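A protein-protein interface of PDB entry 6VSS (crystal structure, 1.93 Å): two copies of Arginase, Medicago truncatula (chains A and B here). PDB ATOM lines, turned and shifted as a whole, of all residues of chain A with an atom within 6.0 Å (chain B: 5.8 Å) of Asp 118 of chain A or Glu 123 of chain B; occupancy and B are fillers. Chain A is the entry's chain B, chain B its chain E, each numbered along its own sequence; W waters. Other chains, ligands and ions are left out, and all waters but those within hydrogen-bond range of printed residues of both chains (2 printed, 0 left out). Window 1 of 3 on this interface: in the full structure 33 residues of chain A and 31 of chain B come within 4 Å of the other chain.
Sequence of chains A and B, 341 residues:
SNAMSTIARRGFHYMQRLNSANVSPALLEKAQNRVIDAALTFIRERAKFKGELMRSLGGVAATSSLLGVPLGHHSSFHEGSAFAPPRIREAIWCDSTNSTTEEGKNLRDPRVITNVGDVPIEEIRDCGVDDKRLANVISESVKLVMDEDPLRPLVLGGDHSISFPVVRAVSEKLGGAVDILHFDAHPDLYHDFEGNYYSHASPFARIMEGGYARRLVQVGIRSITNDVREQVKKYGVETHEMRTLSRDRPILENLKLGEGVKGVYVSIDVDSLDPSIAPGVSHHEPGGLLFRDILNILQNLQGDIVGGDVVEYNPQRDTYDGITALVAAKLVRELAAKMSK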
ATOM      1  N   PHE A  42      14.875 -29.123   5.528  1.00  0.00           N
ATOM      2  CA  PHE A  42      13.834 -29.253   4.470  1.00  0.00           C
ATOM      3  C   PHE A  42      13.381 -27.840   4.081  1.00  0.00           C
ATOM      4  O   PHE A  42      13.343 -27.509   2.847  1.00  0.00           O
ATOM      5  CB  PHE A  42      12.619 -30.073   4.919  1.00  0.00           C
ATOM      6  CG  PHE A  42      11.544 -30.181   3.876  1.00  0.00           C
ATOM      7  CD1 PHE A  42      11.677 -31.057   2.808  1.00  0.00           C
ATOM      8  CD2 PHE A  42      10.400 -29.435   3.958  1.00  0.00           C
ATOM      9  CE1 PHE A  42      10.682 -31.179   1.845  1.00  0.00           C
ATOM     10  CE2 PHE A  42       9.407 -29.550   3.001  1.00  0.00           C
ATOM     11  CZ  PHE A  42       9.560 -30.406   1.940  1.00  0.00           C
ATOM     12  N   ILE A  43      13.031 -27.034   5.096  1.00  0.00           N
ATOM     13  CA  ILE A  43      12.599 -25.612   4.908  1.00  0.00           C
ATOM     14  C   ILE A  43      13.753 -24.869   4.226  1.00  0.00           C
ATOM     15  O   ILE A  43      13.489 -24.128   3.301  1.00  0.00           O
ATOM     16  CB  ILE A  43      12.129 -24.887   6.210  1.00  0.00           C
ATOM     17  CG1 ILE A  43      10.979 -25.579   6.957  1.00  0.00           C
ATOM     18  CG2 ILE A  43      11.795 -23.425   5.920  1.00  0.00           C
ATOM     19  CD1 ILE A  43       9.617 -25.487   6.297  1.00  0.00           C
ATOM     20  N   ARG A  46      13.675 -25.743   0.500  1.00  0.00           N
ATOM     21  CA  ARG A  46      12.530 -25.195  -0.270  1.00  0.00           C
ATOM     22  C   ARG A  46      12.755 -23.698  -0.424  1.00  0.00           C
ATOM     23  O   ARG A  46      12.491 -23.175  -1.523  1.00  0.00           O
ATOM     24  CB  ARG A  46      11.214 -25.592   0.391  1.00  0.00           C
ATOM     25  CG  ARG A  46      10.914 -27.064   0.182  1.00  0.00           C
ATOM     26  CD  ARG A  46      10.125 -27.297  -1.100  1.00  0.00           C
ATOM     27  NE  ARG A  46       8.913 -26.511  -1.224  1.00  0.00           N
ATOM     28  CZ  ARG A  46       8.345 -26.186  -2.377  1.00  0.00           C
ATOM     29  NH1 ARG A  46       8.825 -26.655  -3.529  1.00  0.00           N
ATOM     30  NH2 ARG A  46       7.247 -25.450  -2.368  1.00  0.00           N
ATOM     31  N   LEU A  66       4.848 -18.442   1.205  1.00  0.00           N
ATOM     32  CA  LEU A  66       3.965 -19.108   2.168  1.00  0.00           C
ATOM     33  C   LEU A  66       4.814 -20.047   3.006  1.00  0.00           C
ATOM     34  O   LEU A  66       5.426 -20.958   2.470  1.00  0.00           O
ATOM     35  CB  LEU A  66       2.856 -19.843   1.418  1.00  0.00           C
ATOM     36  CG  LEU A  66       2.091 -18.976   0.436  1.00  0.00           C
ATOM     37  CD1 LEU A  66       0.817 -19.658  -0.057  1.00  0.00           C
ATOM     38  CD2 LEU A  66       1.752 -17.677   1.090  1.00  0.00           C
ATOM     39  N   LEU A  67       4.772 -19.852   4.309  1.00  0.00           N
ATOM     40  CA  LEU A  67       5.269 -20.803   5.336  1.00  0.00           C
ATOM     41  C   LEU A  67       4.097 -21.191   6.228  1.00  0.00           C
ATOM     42  O   LEU A  67       3.533 -20.302   6.903  1.00  0.00           O
ATOM     43  CB  LEU A  67       6.425 -20.124   6.091  1.00  0.00           C
ATOM     44  CG  LEU A  67       7.114 -20.975   7.142  1.00  0.00           C
ATOM     45  CD1 LEU A  67       8.097 -21.934   6.482  1.00  0.00           C
ATOM     46  CD2 LEU A  67       7.818 -20.105   8.170  1.00  0.00           C
ATOM     47  N   GLY A  68       3.673 -22.450   6.131  1.00  0.00           N
ATOM     48  CA  GLY A  68       2.699 -23.102   7.005  1.00  0.00           C
ATOM     49  C   GLY A  68       3.284 -23.405   8.376  1.00  0.00           C
ATOM     50  O   GLY A  68       4.459 -23.895   8.476  1.00  0.00           O
ATOM     51  N   VAL A  69       2.490 -23.081   9.406  1.00  0.00           N
ATOM     52  CA  VAL A  69       2.751 -23.499  10.811  1.00  0.00           C
ATOM     53  C   VAL A  69       1.452 -24.117  11.316  1.00  0.00           C
ATOM     54  O   VAL A  69       0.610 -23.417  11.888  1.00  0.00           O
ATOM     55  CB  VAL A  69       3.248 -22.310  11.642  1.00  0.00           C
ATOM     56  CG1 VAL A  69       3.665 -22.761  13.025  1.00  0.00           C
ATOM     57  CG2 VAL A  69       4.369 -21.558  10.932  1.00  0.00           C
ATOM     58  N   PRO A  70       1.257 -25.426  10.984  1.00  0.00           N
ATOM     59  CA  PRO A  70       0.060 -26.189  11.341  1.00  0.00           C
ATOM     60  C   PRO A  70       0.055 -26.613  12.822  1.00  0.00           C
ATOM     61  O   PRO A  70       0.295 -27.724  13.117  1.00  0.00           O
ATOM     62  CB  PRO A  70       0.160 -27.395  10.411  1.00  0.00           C
ATOM     63  CG  PRO A  70       1.670 -27.590  10.260  1.00  0.00           C
ATOM     64  CD  PRO A  70       2.213 -26.192  10.160  1.00  0.00           C
ATOM     65  N   PRO A  85      -3.283 -24.826   6.806  1.00  0.00           N
ATOM     66  CA  PRO A  85      -2.451 -24.348   5.711  1.00  0.00           C
ATOM     67  C   PRO A  85      -2.677 -25.054   4.358  1.00  0.00           C
ATOM     68  O   PRO A  85      -2.838 -24.348   3.372  1.00  0.00           O
ATOM     69  CB  PRO A  85      -1.037 -24.434   6.285  1.00  0.00           C
ATOM     70  CG  PRO A  85      -1.226 -24.287   7.776  1.00  0.00           C
ATOM     71  CD  PRO A  85      -2.512 -25.049   8.032  1.00  0.00           C
ATOM     72  N   PRO A  86      -2.701 -26.409   4.240  1.00  0.00           N
ATOM     73  CA  PRO A  86      -2.881 -27.101   2.958  1.00  0.00           C
ATOM     74  C   PRO A  86      -4.244 -26.802   2.323  1.00  0.00           C
ATOM     75  O   PRO A  86      -4.320 -26.733   1.103  1.00  0.00           O
ATOM     76  CB  PRO A  86      -2.844 -28.604   3.301  1.00  0.00           C
ATOM     77  CG  PRO A  86      -2.039 -28.635   4.581  1.00  0.00           C
ATOM     78  CD  PRO A  86      -2.453 -27.367   5.313  1.00  0.00           C
ATOM     79  N   ARG A  89      -3.744 -23.259   0.735  1.00  0.00           N
ATOM     80  CA  ARG A  89      -3.038 -23.326  -0.580  1.00  0.00           C
ATOM     81  C   ARG A  89      -3.966 -23.890  -1.661  1.00  0.00           C
ATOM     82  O   ARG A  89      -3.916 -23.454  -2.799  1.00  0.00           O
ATOM     83  CB  ARG A  89      -1.749 -24.122  -0.501  1.00  0.00           C
ATOM     84  CG  ARG A  89      -0.758 -23.458   0.434  1.00  0.00           C
ATOM     85  CD  ARG A  89       0.561 -24.132   0.456  1.00  0.00           C
ATOM     86  NE  ARG A  89       0.376 -25.406   1.099  1.00  0.00           N
ATOM     87  CZ  ARG A  89       0.630 -25.643   2.393  1.00  0.00           C
ATOM     88  NH1 ARG A  89       1.146 -24.706   3.154  1.00  0.00           N
ATOM     89  NH2 ARG A  89       0.466 -26.838   2.884  1.00  0.00           N
ATOM     90  N   ASN A 115       4.959 -20.877  -2.715  1.00  0.00           N
ATOM     91  CA  ASN A 115       4.878 -21.754  -1.525  1.00  0.00           C
ATOM     92  C   ASN A 115       6.283 -22.187  -1.117  1.00  0.00           C
ATOM     93  O   ASN A 115       6.982 -22.685  -1.962  1.00  0.00           O
ATOM     94  CB  ASN A 115       4.021 -22.980  -1.796  1.00  0.00           C
ATOM     95  CG  ASN A 115       3.824 -23.799  -0.535  1.00  0.00           C
ATOM     96  OD1 ASN A 115       3.795 -23.275   0.588  1.00  0.00           O
ATOM     97  ND2 ASN A 115       3.721 -25.098  -0.697  1.00  0.00           N
ATOM     98  N   VAL A 116       6.652 -22.064   0.140  1.00  0.00           N
ATOM     99  CA  VAL A 116       7.904 -22.663   0.675  1.00  0.00           C
ATOM    100  C   VAL A 116       7.517 -24.008   1.291  1.00  0.00           C
ATOM    101  O   VAL A 116       7.904 -25.036   0.736  1.00  0.00           O
ATOM    102  CB  VAL A 116       8.600 -21.740   1.687  1.00  0.00           C
ATOM    103  CG1 VAL A 116       9.659 -22.480   2.500  1.00  0.00           C
ATOM    104  CG2 VAL A 116       9.210 -20.521   1.015  1.00  0.00           C
ATOM    105  N   GLY A 117       6.644 -24.006   2.302  1.00  0.00           N
ATOM    106  CA  GLY A 117       6.057 -25.251   2.829  1.00  0.00           C
ATOM    107  C   GLY A 117       5.673 -25.136   4.288  1.00  0.00           C
ATOM    108  O   GLY A 117       5.523 -24.029   4.750  1.00  0.00           O
ATOM    109  N   ASP A 118       5.459 -26.273   4.946  1.00  0.00           N
ATOM    110  CA  ASP A 118       4.881 -26.361   6.282  1.00  0.00           C
ATOM    111  C   ASP A 118       6.011 -26.798   7.207  1.00  0.00           C
ATOM    112  O   ASP A 118       6.727 -27.741   6.867  1.00  0.00           O
ATOM    113  CB  ASP A 118       3.687 -27.317   6.303  1.00  0.00           C
ATOM    114  CG  ASP A 118       2.448 -26.785   5.625  1.00  0.00           C
ATOM    115  OD1 ASP A 118       2.497 -25.697   5.068  1.00  0.00           O
ATOM    116  OD2 ASP A 118       1.436 -27.465   5.678  1.00  0.00           O
ATOM    117  N   VAL A 119       6.178 -26.104   8.320  1.00  0.00           N
ATOM    118  CA  VAL A 119       6.932 -26.641   9.482  1.00  0.00           C
ATOM    119  C   VAL A 119       6.144 -27.835  10.022  1.00  0.00           C
ATOM    120  O   VAL A 119       5.011 -27.640  10.457  1.00  0.00           O
ATOM    121  CB  VAL A 119       7.111 -25.613  10.603  1.00  0.00           C
ATOM    122  CG1 VAL A 119       7.828 -26.245  11.804  1.00  0.00           C
ATOM    123  CG2 VAL A 119       7.817 -24.359  10.096  1.00  0.00           C
ATOM    124  N   PRO A 120       6.756 -29.044  10.073  1.00  0.00           N
ATOM    125  CA  PRO A 120       6.104 -30.271  10.553  1.00  0.00           C
ATOM    126  C   PRO A 120       5.957 -30.351  12.078  1.00  0.00           C
ATOM    127  O   PRO A 120       6.681 -31.110  12.803  1.00  0.00           O
ATOM    128  CB  PRO A 120       7.041 -31.370  10.033  1.00  0.00           C
ATOM    129  CG  PRO A 120       8.403 -30.723  10.030  1.00  0.00           C
ATOM    130  CD  PRO A 120       8.148 -29.274   9.658  1.00  0.00           C
ATOM    131  N   LEU A 156       1.094 -19.035   7.130  1.00  0.00           N
ATOM    132  CA  LEU A 156      -0.291 -19.581   7.259  1.00  0.00           C
ATOM    133  C   LEU A 156      -0.400 -20.377   8.553  1.00  0.00           C
ATOM    134  O   LEU A 156       0.440 -21.323   8.749  1.00  0.00           O
ATOM    135  CB  LEU A 156      -0.601 -20.503   6.102  1.00  0.00           C
ATOM    136  CG  LEU A 156      -0.366 -19.916   4.733  1.00  0.00           C
ATOM    137  CD1 LEU A 156      -0.646 -21.001   3.730  1.00  0.00           C
ATOM    138  CD2 LEU A 156      -1.237 -18.693   4.507  1.00  0.00           C
ATOM    139  N   VAL B  35      15.580 -31.238  -2.381  1.00  0.00           N
ATOM    140  CA  VAL B  35      14.286 -31.292  -1.627  1.00  0.00           C
ATOM    141  C   VAL B  35      13.922 -32.772  -1.330  1.00  0.00           C
ATOM    142  O   VAL B  35      13.541 -33.103  -0.190  1.00  0.00           O
ATOM    143  CB  VAL B  35      13.154 -30.537  -2.371  1.00  0.00           C
ATOM    144  CG1 VAL B  35      11.770 -30.826  -1.776  1.00  0.00           C
ATOM    145  CG2 VAL B  35      13.403 -29.031  -2.391  1.00  0.00           C
ATOM    146  N   PRO B 120       6.241 -35.381   2.147  1.00  0.00           N
ATOM    147  CA  PRO B 120       5.747 -34.057   1.803  1.00  0.00           C
ATOM    148  C   PRO B 120       5.466 -33.945   0.313  1.00  0.00           C
ATOM    149  O   PRO B 120       6.230 -33.284  -0.430  1.00  0.00           O
ATOM    150  CB  PRO B 120       6.857 -33.150   2.373  1.00  0.00           C
ATOM    151  CG  PRO B 120       8.109 -33.962   2.243  1.00  0.00           C
ATOM    152  CD  PRO B 120       7.684 -35.380   2.509  1.00  0.00           C
ATOM    153  N   ILE B 121       4.313 -34.504  -0.079  1.00  0.00           N
ATOM    154  CA  ILE B 121       3.997 -34.772  -1.506  1.00  0.00           C
ATOM    155  C   ILE B 121       3.894 -33.446  -2.274  1.00  0.00           C
ATOM    156  O   ILE B 121       4.456 -33.360  -3.381  1.00  0.00           O
ATOM    157  CB  ILE B 121       2.689 -35.580  -1.626  1.00  0.00           C
ATOM    158  CG1 ILE B 121       2.836 -36.995  -1.033  1.00  0.00           C
ATOM    159  CG2 ILE B 121       2.203 -35.582  -3.074  1.00  0.00           C
ATOM    160  CD1 ILE B 121       3.829 -37.936  -1.786  1.00  0.00           C
ATOM    161  N   GLU B 122       3.092 -32.514  -1.756  1.00  0.00           N
ATOM    162  CA  GLU B 122       2.803 -31.163  -2.318  1.00  0.00           C
ATOM    163  C   GLU B 122       4.161 -30.471  -2.600  1.00  0.00           C
ATOM    164  O   GLU B 122       4.394 -30.007  -3.721  1.00  0.00           O
ATOM    165  CB  GLU B 122       1.923 -30.390  -1.315  1.00  0.00           C
ATOM    166  CG  GLU B 122       1.226 -29.150  -1.870  1.00  0.00           C
ATOM    167  CD  GLU B 122       0.504 -28.223  -0.861  1.00  0.00           C
ATOM    168  OE1 GLU B 122       0.196 -28.618   0.336  1.00  0.00           O
ATOM    169  OE2 GLU B 122       0.234 -27.043  -1.254  1.00  0.00           O
ATOM    170  N   GLU B 123       5.059 -30.479  -1.623  1.00  0.00           N
ATOM    171  CA  GLU B 123       6.373 -29.772  -1.688  1.00  0.00           C
ATOM    172  C   GLU B 123       7.318 -30.474  -2.667  1.00  0.00           C
ATOM    173  O   GLU B 123       8.062 -29.796  -3.288  1.00  0.00           O
ATOM    174  CB  GLU B 123       6.950 -29.643  -0.284  1.00  0.00           C
ATOM    175  CG  GLU B 123       6.102 -28.705   0.588  1.00  0.00           C
ATOM    176  CD  GLU B 123       5.055 -29.347   1.500  1.00  0.00           C
ATOM    177  OE1 GLU B 123       4.629 -30.504   1.235  1.00  0.00           O
ATOM    178  OE2 GLU B 123       4.645 -28.672   2.487  1.00  0.00           O
ATOM    179  N   ILE B 124       7.236 -31.782  -2.856  1.00  0.00           N
ATOM    180  CA  ILE B 124       8.085 -32.503  -3.840  1.00  0.00           C
ATOM    181  C   ILE B 124       7.473 -32.260  -5.228  1.00  0.00           C
ATOM    182  O   ILE B 124       8.225 -31.819  -6.119  1.00  0.00           O
ATOM    183  CB  ILE B 124       8.259 -33.972  -3.412  1.00  0.00           C
ATOM    184  CG1 ILE B 124       9.182 -34.054  -2.187  1.00  0.00           C
ATOM    185  CG2 ILE B 124       8.788 -34.846  -4.532  1.00  0.00           C
ATOM    186  CD1 ILE B 124       8.991 -35.289  -1.342  1.00  0.00           C
ATOM    187  N   ARG B 125       6.150 -32.341  -5.397  1.00  0.00           N
ATOM    188  CA  ARG B 125       5.519 -32.097  -6.730  1.00  0.00           C
ATOM    189  C   ARG B 125       5.809 -30.672  -7.230  1.00  0.00           C
ATOM    190  O   ARG B 125       5.986 -30.465  -8.443  1.00  0.00           O
ATOM    191  CB  ARG B 125       3.998 -32.225  -6.690  1.00  0.00           C
ATOM    192  CG  ARG B 125       3.483 -33.622  -6.422  1.00  0.00           C
ATOM    193  CD  ARG B 125       2.407 -33.915  -7.437  1.00  0.00           C
ATOM    194  NE  ARG B 125       1.303 -32.971  -7.449  1.00  0.00           N
ATOM    195  CZ  ARG B 125       0.553 -32.664  -8.508  1.00  0.00           C
ATOM    196  NH1 ARG B 125       0.833 -33.140  -9.704  1.00  0.00           N
ATOM    197  NH2 ARG B 125      -0.475 -31.846  -8.378  1.00  0.00           N
ATOM    198  N   ASP B 126       5.818 -29.716  -6.314  1.00  0.00           N
ATOM    199  CA  ASP B 126       6.018 -28.279  -6.609  1.00  0.00           C
ATOM    200  C   ASP B 126       7.482 -27.988  -7.025  1.00  0.00           C
ATOM    201  O   ASP B 126       7.734 -26.856  -7.380  1.00  0.00           O
ATOM    202  CB  ASP B 126       5.556 -27.461  -5.404  1.00  0.00           C
ATOM    203  CG  ASP B 126       5.754 -25.975  -5.601  1.00  0.00           C
ATOM    204  OD1 ASP B 126       5.142 -25.454  -6.535  1.00  0.00           O
ATOM    205  OD2 ASP B 126       6.567 -25.394  -4.871  1.00  0.00           O
ATOM    206  N   CYS B 127       8.409 -28.950  -6.980  1.00  0.00           N
ATOM    207  CA  CYS B 127       9.761 -28.892  -7.622  1.00  0.00           C
ATOM    208  C   CYS B 127       9.780 -29.455  -9.056  1.00  0.00           C
ATOM    209  O   CYS B 127      10.863 -29.459  -9.647  1.00  0.00           O
ATOM    210  CB  CYS B 127      10.769 -29.704  -6.816  1.00  0.00           C
ATOM    211  SG  CYS B 127      10.879 -29.123  -5.118  1.00  0.00           S
HETATM  212  O   HOH W   1       2.699 -30.148   4.050  1.00  0.00           O
HETATM  213  O   HOH W   2      -2.641 -28.143  -0.644  1.00  0.00           O
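The guanidinium group (NH1) of Arg 46 of chain A lies within hydrogen-bond range of the backbone carbonyl oxygen (O) of Glu 123 of chain B (3.2 Å).
The guanidinium group (NH2) of Arg 46 of chain A is in salt-bridge range of the side-chain carboxylate (OD2) of Asp 126 of chain B (2.6 Å).
NH1 of Arg 46 of chain A lies within hydrogen-bond range of SG of Cys 127 of chain B (3.6 Å).
NE of Arg 89 of chain A is in salt-bridge range of OE2 of Glu 122 of chain B (2.9 Å).
The backbone carbonyl oxygen (O) of Asn 115 of chain A lies within hydrogen-bond range of the guanidinium group (NH2) of Arg 46 of chain A (2.8 Å).
The side-chain amide oxygen (OD1) of Asn 115 of chain A lies within hydrogen-bond range of the backbone NH (N) of Gly 117 of chain A.
N of Gly 117 of chain A lies within hydrogen-bond range of O of Leu 66 of chain A (3.3 Å).
The guanidinium group (NE) of Arg 46 of chain A sits at hydrogen-bond distance from the backbone carbonyl oxygen (O) of Val 116 of chain A (2.7 Å).
O of Leu 66 of chain A lies close to OD1 of Asn 115 of chain A, 3.4 Å away.
The guanidinium group of Arg 89 of chain A is in salt-bridge range of the side-chain carboxylate of Asp 118 of chain A, at 2.5 Å.
Val 35 of chain B touches Phe 42 of chain A (CG1 to CE1, 3.8 Å).
Pro 120 of chain B touches Phe 42 of chain A (CG to CE1, 3.8 Å).
Glu 123 of chain B touches Phe 42 of chain A (CB to CZ, 3.5 Å).
CG2 of Val 35 of chain B touches CD of Arg 46 of chain A (3.9 Å).
Asp 126 of chain B touches Asn 115 of chain A (OD2 to O, 3.997 Å).
Glu 123 of chain B touches Gly 117 of chain A.
Glu 123 of chain B touches Asp 118 of chain A.
Asp 118 of chain A touches one residue of chain B.
Glu 123 of chain B touches just these residues of chain A: Phe 42 (3.5 Å), Arg 46 (3.2 Å), Gly 117 (3.7 Å) and Asp 118 (3.5 Å).
Printed residues of chain B within 4 Å of Arg 89 of chain A: Glu 122 (2.9 Å).
Of the printed residues of chain B, Phe 42 of chain A touches Val 35, Pro 120 and Glu 123.
Printed residues of chain A within 4 Å of Val 35 of chain B: Phe 42 and Arg 46.
Ile 43 of chain A touches none of the printed residues of chain B.
The nearest residue of chain B that does not touch Asp 118 of chain A is Glu 122 of chain B (5.6 Å).
The nearest residue of chain A that does not touch Glu 123 of chain B is Val 116 of chain A (4.1 Å).
Of the 9 printed residues of chain B, 6 touch a printed residue of chain A.
Of the 18 printed residues of chain A, 6 touch a printed residue of chain B.
Hydrophobic or aromatic side chains of chain A that line the printed part of chain B: Phe 42.
Among the printed residues, Asp or Glu carboxylates within 4 Å of a Lys or Arg side-chain nitrogen of the other chain: Arg 46 of chain A with Asp 126 of chain B and Arg 89 of chain A with Glu 122 of chain B.
Position printed for both chains: 120.
Water W2 lies within hydrogen-bond range of O of Pro 86 of chain A (2.8 Å) and OE1 of Glu 122 of chain B (3.0 Å).
Water W1 lies within hydrogen-bond range of the side-chain carboxylate of Glu 123 of chain B (2.9 Å) and the side-chain carboxylate of Asp 118 of chain A (3.4 Å).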
